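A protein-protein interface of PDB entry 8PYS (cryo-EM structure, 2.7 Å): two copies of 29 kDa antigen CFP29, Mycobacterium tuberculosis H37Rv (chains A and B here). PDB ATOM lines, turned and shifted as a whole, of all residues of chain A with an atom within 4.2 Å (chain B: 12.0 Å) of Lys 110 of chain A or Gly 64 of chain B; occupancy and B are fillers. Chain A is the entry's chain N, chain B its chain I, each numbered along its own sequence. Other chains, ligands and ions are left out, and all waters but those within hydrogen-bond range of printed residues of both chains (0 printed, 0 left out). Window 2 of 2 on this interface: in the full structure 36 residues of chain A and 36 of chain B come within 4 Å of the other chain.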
ATOM      1  N   VAL A  80      18.915  30.891   2.402  1.00  0.00           N
ATOM      2  CA  VAL A  80      17.680  31.033   3.167  1.00  0.00           C
ATOM      3  C   VAL A  80      17.216  32.481   3.078  1.00  0.00           C
ATOM      4  O   VAL A  80      17.712  33.340   3.820  1.00  0.00           O
ATOM      5  CB  VAL A  80      17.871  30.592   4.624  1.00  0.00           C
ATOM      6  CG1 VAL A  80      16.549  30.640   5.364  1.00  0.00           C
ATOM      7  CG2 VAL A  80      18.454  29.196   4.674  1.00  0.00           C
ATOM      8  N   PRO A  81      16.291  32.802   2.180  1.00  0.00           N
ATOM      9  CA  PRO A  81      15.783  34.173   2.107  1.00  0.00           C
ATOM     10  C   PRO A  81      14.941  34.530   3.322  1.00  0.00           C
ATOM     11  O   PRO A  81      14.279  33.683   3.923  1.00  0.00           O
ATOM     12  CB  PRO A  81      14.939  34.171   0.828  1.00  0.00           C
ATOM     13  CG  PRO A  81      14.533  32.758   0.654  1.00  0.00           C
ATOM     14  CD  PRO A  81      15.658  31.923   1.183  1.00  0.00           C
ATOM     15  N   GLU A 106      14.943  33.334  12.478  1.00  0.00           N
ATOM     16  CA  GLU A 106      14.356  32.172  11.822  1.00  0.00           C
ATOM     17  C   GLU A 106      15.226  31.690  10.670  1.00  0.00           C
ATOM     18  O   GLU A 106      15.451  30.484  10.517  1.00  0.00           O
ATOM     19  CB  GLU A 106      12.950  32.513  11.327  1.00  0.00           C
ATOM     20  CG  GLU A 106      12.211  31.350  10.696  1.00  0.00           C
ATOM     21  CD  GLU A 106      10.893  31.764  10.067  1.00  0.00           C
ATOM     22  OE1 GLU A 106      10.603  32.978  10.031  1.00  0.00           O
ATOM     23  OE2 GLU A 106      10.147  30.874   9.611  1.00  0.00           O
ATOM     24  N   ALA A 107      15.734  32.615   9.853  1.00  0.00           N
ATOM     25  CA  ALA A 107      16.591  32.227   8.741  1.00  0.00           C
ATOM     26  C   ALA A 107      17.893  31.611   9.233  1.00  0.00           C
ATOM     27  O   ALA A 107      18.374  30.623   8.666  1.00  0.00           O
ATOM     28  CB  ALA A 107      16.871  33.433   7.847  1.00  0.00           C
ATOM     29  N   ALA A 108      18.484  32.183  10.284  1.00  0.00           N
ATOM     30  CA  ALA A 108      19.729  31.646  10.820  1.00  0.00           C
ATOM     31  C   ALA A 108      19.523  30.258  11.409  1.00  0.00           C
ATOM     32  O   ALA A 108      20.347  29.359  11.203  1.00  0.00           O
ATOM     33  CB  ALA A 108      20.302  32.600  11.864  1.00  0.00           C
ATOM     34  N   LYS A 109      18.422  30.058  12.137  1.00  0.00           N
ATOM     35  CA  LYS A 109      18.128  28.737  12.679  1.00  0.00           C
ATOM     36  C   LYS A 109      17.875  27.733  11.566  1.00  0.00           C
ATOM     37  O   LYS A 109      18.301  26.578  11.657  1.00  0.00           O
ATOM     38  CB  LYS A 109      16.926  28.801  13.619  1.00  0.00           C
ATOM     39  CG  LYS A 109      16.627  27.474  14.293  1.00  0.00           C
ATOM     40  CD  LYS A 109      15.577  27.599  15.379  1.00  0.00           C
ATOM     41  CE  LYS A 109      14.198  27.792  14.784  1.00  0.00           C
ATOM     42  NZ  LYS A 109      13.133  27.665  15.812  1.00  0.00           N
ATOM     43  N   LYS A 110      17.183  28.153  10.506  1.00  0.00           N
ATOM     44  CA  LYS A 110      16.917  27.253   9.389  1.00  0.00           C
ATOM     45  C   LYS A 110      18.207  26.860   8.677  1.00  0.00           C
ATOM     46  O   LYS A 110      18.397  25.691   8.324  1.00  0.00           O
ATOM     47  CB  LYS A 110      15.932  27.911   8.422  1.00  0.00           C
ATOM     48  CG  LYS A 110      15.471  27.013   7.295  1.00  0.00           C
ATOM     49  CD  LYS A 110      14.919  27.833   6.143  1.00  0.00           C
ATOM     50  CE  LYS A 110      13.828  28.783   6.611  1.00  0.00           C
ATOM     51  NZ  LYS A 110      13.165  29.498   5.486  1.00  0.00           N
ATOM     52  N   LEU A 111      19.110  27.821   8.465  1.00  0.00           N
ATOM     53  CA  LEU A 111      20.392  27.504   7.844  1.00  0.00           C
ATOM     54  C   LEU A 111      21.220  26.577   8.726  1.00  0.00           C
ATOM     55  O   LEU A 111      21.851  25.636   8.229  1.00  0.00           O
ATOM     56  CB  LEU A 111      21.167  28.786   7.540  1.00  0.00           C
ATOM     57  CG  LEU A 111      22.404  28.605   6.651  1.00  0.00           C
ATOM     58  CD1 LEU A 111      22.000  28.156   5.257  1.00  0.00           C
ATOM     59  CD2 LEU A 111      23.225  29.880   6.583  1.00  0.00           C
ATOM     60  N   ALA A 112      21.236  26.828  10.038  1.00  0.00           N
ATOM     61  CA  ALA A 112      21.964  25.952  10.948  1.00  0.00           C
ATOM     62  C   ALA A 112      21.384  24.543  10.940  1.00  0.00           C
ATOM     63  O   ALA A 112      22.128  23.555  10.969  1.00  0.00           O
ATOM     64  CB  ALA A 112      21.950  26.530  12.362  1.00  0.00           C
ATOM     65  N   PHE A 113      20.055  24.432  10.901  1.00  0.00           N
ATOM     66  CA  PHE A 113      19.421  23.121  10.853  1.00  0.00           C
ATOM     67  C   PHE A 113      19.770  22.390   9.566  1.00  0.00           C
ATOM     68  O   PHE A 113      20.053  21.188   9.587  1.00  0.00           O
ATOM     69  CB  PHE A 113      17.906  23.257  10.993  1.00  0.00           C
ATOM     70  CG  PHE A 113      17.433  23.371  12.415  1.00  0.00           C
ATOM     71  CD1 PHE A 113      18.290  23.798  13.415  1.00  0.00           C
ATOM     72  CD2 PHE A 113      16.137  23.028  12.755  1.00  0.00           C
ATOM     73  CE1 PHE A 113      17.858  23.898  14.716  1.00  0.00           C
ATOM     74  CE2 PHE A 113      15.702  23.124  14.059  1.00  0.00           C
ATOM     75  CZ  PHE A 113      16.564  23.558  15.040  1.00  0.00           C
ATOM     76  N   VAL A 114      19.753  23.097   8.437  1.00  0.00           N
ATOM     77  CA  VAL A 114      20.098  22.470   7.164  1.00  0.00           C
ATOM     78  C   VAL A 114      21.544  21.994   7.182  1.00  0.00           C
ATOM     79  O   VAL A 114      21.847  20.878   6.748  1.00  0.00           O
ATOM     80  CB  VAL A 114      19.826  23.437   5.998  1.00  0.00           C
ATOM     81  CG1 VAL A 114      20.489  22.940   4.730  1.00  0.00           C
ATOM     82  CG2 VAL A 114      18.335  23.592   5.785  1.00  0.00           C
ATOM     83  N   VAL B  58      19.030  21.951  -7.588  1.00  0.00           N
ATOM     84  CA  VAL B  58      18.890  20.677  -6.897  1.00  0.00           C
ATOM     85  C   VAL B  58      17.727  20.795  -5.924  1.00  0.00           C
ATOM     86  O   VAL B  58      17.363  21.893  -5.494  1.00  0.00           O
ATOM     87  CB  VAL B  58      20.202  20.275  -6.177  1.00  0.00           C
ATOM     88  CG1 VAL B  58      20.502  21.219  -5.029  1.00  0.00           C
ATOM     89  CG2 VAL B  58      20.153  18.830  -5.702  1.00  0.00           C
ATOM     90  N   LYS B  59      17.100  19.662  -5.596  1.00  0.00           N
ATOM     91  CA  LYS B  59      15.914  19.659  -4.728  1.00  0.00           C
ATOM     92  C   LYS B  59      16.211  19.972  -3.280  1.00  0.00           C
ATOM     93  O   LYS B  59      16.721  19.126  -2.571  1.00  0.00           O
ATOM     94  CB  LYS B  59      15.244  18.280  -4.824  1.00  0.00           C
ATOM     95  CG  LYS B  59      13.944  18.076  -4.050  1.00  0.00           C
ATOM     96  CD  LYS B  59      13.392  16.681  -4.294  1.00  0.00           C
ATOM     97  CE  LYS B  59      12.107  16.411  -3.528  1.00  0.00           C
ATOM     98  NZ  LYS B  59      11.591  15.041  -3.784  1.00  0.00           N
ATOM     99  N   ALA B  60      15.819  21.151  -2.818  1.00  0.00           N
ATOM    100  CA  ALA B  60      16.121  21.574  -1.447  1.00  0.00           C
ATOM    101  C   ALA B  60      15.975  20.498  -0.366  1.00  0.00           C
ATOM    102  O   ALA B  60      15.112  19.629  -0.472  1.00  0.00           O
ATOM    103  CB  ALA B  60      15.258  22.767  -1.083  1.00  0.00           C
ATOM    104  N   PRO B  61      16.783  20.579   0.701  1.00  0.00           N
ATOM    105  CA  PRO B  61      16.773  19.604   1.797  1.00  0.00           C
ATOM    106  C   PRO B  61      15.612  19.833   2.752  1.00  0.00           C
ATOM    107  O   PRO B  61      15.004  18.878   3.243  1.00  0.00           O
ATOM    108  CB  PRO B  61      18.126  19.835   2.482  1.00  0.00           C
ATOM    109  CG  PRO B  61      18.470  21.246   2.176  1.00  0.00           C
ATOM    110  CD  PRO B  61      17.844  21.589   0.855  1.00  0.00           C
ATOM    111  N   THR B  62      15.293  21.098   3.017  1.00  0.00           N
ATOM    112  CA  THR B  62      14.173  21.467   3.869  1.00  0.00           C
ATOM    113  C   THR B  62      13.383  22.574   3.183  1.00  0.00           C
ATOM    114  O   THR B  62      13.835  23.180   2.210  1.00  0.00           O
ATOM    115  CB  THR B  62      14.624  21.926   5.266  1.00  0.00           C
ATOM    116  OG1 THR B  62      15.224  23.224   5.180  1.00  0.00           O
ATOM    117  CG2 THR B  62      15.620  20.946   5.876  1.00  0.00           C
ATOM    118  N   ASN B  63      12.183  22.823   3.699  1.00  0.00           N
ATOM    119  CA  ASN B  63      11.349  23.890   3.169  1.00  0.00           C
ATOM    120  C   ASN B  63      11.955  25.254   3.483  1.00  0.00           C
ATOM    121  O   ASN B  63      12.596  25.452   4.518  1.00  0.00           O
ATOM    122  CB  ASN B  63       9.938  23.798   3.750  1.00  0.00           C
ATOM    123  CG  ASN B  63       8.940  24.650   2.993  1.00  0.00           C
ATOM    124  OD1 ASN B  63       9.016  24.779   1.772  1.00  0.00           O
ATOM    125  ND2 ASN B  63       7.997  25.242   3.720  1.00  0.00           N
ATOM    126  N   GLY B  64      11.749  26.201   2.572  1.00  0.00           N
ATOM    127  CA  GLY B  64      12.259  27.544   2.752  1.00  0.00           C
ATOM    128  C   GLY B  64      13.736  27.712   2.491  1.00  0.00           C
ATOM    129  O   GLY B  64      14.296  28.754   2.842  1.00  0.00           O
ATOM    130  N   VAL B  65      14.386  26.719   1.891  1.00  0.00           N
ATOM    131  CA  VAL B  65      15.810  26.763   1.590  1.00  0.00           C
ATOM    132  C   VAL B  65      15.987  26.524   0.099  1.00  0.00           C
ATOM    133  O   VAL B  65      15.349  25.635  -0.475  1.00  0.00           O
ATOM    134  CB  VAL B  65      16.600  25.719   2.407  1.00  0.00           C
ATOM    135  CG1 VAL B  65      18.062  25.716   1.998  1.00  0.00           C
ATOM    136  CG2 VAL B  65      16.461  25.992   3.891  1.00  0.00           C
ATOM    137  N   ILE B  66      16.834  27.328  -0.532  1.00  0.00           N
ATOM    138  CA  ILE B  66      17.160  27.181  -1.945  1.00  0.00           C
ATOM    139  C   ILE B  66      18.580  26.645  -2.035  1.00  0.00           C
ATOM    140  O   ILE B  66      19.516  27.255  -1.503  1.00  0.00           O
ATOM    141  CB  ILE B  66      17.010  28.507  -2.703  1.00  0.00           C
ATOM    142  CG1 ILE B  66      15.628  29.105  -2.443  1.00  0.00           C
ATOM    143  CG2 ILE B  66      17.211  28.289  -4.190  1.00  0.00           C
ATOM    144  CD1 ILE B  66      15.557  30.592  -2.660  1.00  0.00           C
ATOM    145  N   ALA B  67      18.740  25.506  -2.700  1.00  0.00           N
ATOM    146  CA  ALA B  67      20.017  24.817  -2.782  1.00  0.00           C
ATOM    147  C   ALA B  67      20.472  24.739  -4.229  1.00  0.00           C
ATOM    148  O   ALA B  67      19.667  24.496  -5.132  1.00  0.00           O
ATOM    149  CB  ALA B  67      19.922  23.411  -2.183  1.00  0.00           C
ATOM    150  N   HIS B  68      21.767  24.960  -4.443  1.00  0.00           N
ATOM    151  CA  HIS B  68      22.366  24.925  -5.769  1.00  0.00           C
ATOM    152  C   HIS B  68      23.684  24.172  -5.698  1.00  0.00           C
ATOM    153  O   HIS B  68      24.505  24.441  -4.819  1.00  0.00           O
ATOM    154  CB  HIS B  68      22.606  26.337  -6.308  1.00  0.00           C
ATOM    155  CG  HIS B  68      21.379  26.997  -6.850  1.00  0.00           C
ATOM    156  ND1 HIS B  68      20.634  27.896  -6.120  1.00  0.00           N
ATOM    157  CD2 HIS B  68      20.767  26.891  -8.053  1.00  0.00           C
ATOM    158  CE1 HIS B  68      19.615  28.313  -6.848  1.00  0.00           C
ATOM    159  NE2 HIS B  68      19.673  27.719  -8.024  1.00  0.00           N
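O of Gly 64 of chain B lies within hydrogen-bond range of NZ of Lys 110 of chain A (3.0 Å).
Gly 64 of chain B touches Val 80 of chain A.
Val 65 of chain B touches Val 80 of chain A.
O of Gly 64 of chain B touches CD of Pro 81 of chain A, 3.8 Å away.
Lys 110 of chain A touches Asn 63 of chain B.
Val 65 of chain B touches Lys 110 of chain A.
Val 114 of chain A touches Pro 61 of chain B.
CG2 of Val 114 of chain A touches OG1 of Thr 62 of chain B (3.2 Å).
CG2 of Val 114 of chain A touches CG2 of Val 65 of chain B (3.6 Å).
Printed residues of chain B within 4 Å of Val 80 of chain A: Gly 64 and Val 65.
Pro 81 of chain A touches one residue of chain B.
No residue of chain B comes within 4 Å of Glu 106 of chain A.
No residue of chain B comes within 4 Å of Ala 107 of chain A.
No residue of chain B comes within 4 Å of Lys 109 of chain A.
Lys 110 of chain A touches just these residues of chain B: Asn 63 (3.7 Å), Gly 64 (3.0 Å) and Val 65 (3.3 Å).
No residue of chain B comes within 4 Å of Leu 111 of chain A.
No residue of chain B comes within 4 Å of Phe 113 of chain A.
Val 58 of chain B touches none of the printed residues of chain A.
Printed residues of chain A within 4 Å of Pro 61 of chain B: Val 114.
Of the printed residues of chain A, Thr 62 of chain B touches Val 114 (3.2 Å).
Printed residues of chain A within 4 Å of Asn 63 of chain B: Lys 110 (3.7 Å).
Of chain A, only Val 80, Pro 81 and Lys 110 come within 4 Å of Gly 64 of chain B.
Of the printed residues of chain A, Val 65 of chain B touches Val 80, Lys 110 and Val 114.
The nearest residue of chain B that does not touch Lys 110 of chain A is Thr 62 of chain B (4.3 Å).
Hydrophobic or aromatic side chains of chain A that line the printed part of chain B: Val 80, Pro 81 and Val 114.
Hydrophobic or aromatic side chains of chain B within 4 Å of the printed part of chain A: Pro 61 and Val 65.
Among the printed residues, 9 pairs touch across the chains.
Among the printed residues, no Asp or Glu carboxylate lies within 4 Å of a Lys or Arg side-chain nitrogen of the other chain.
No position is printed for both chains.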
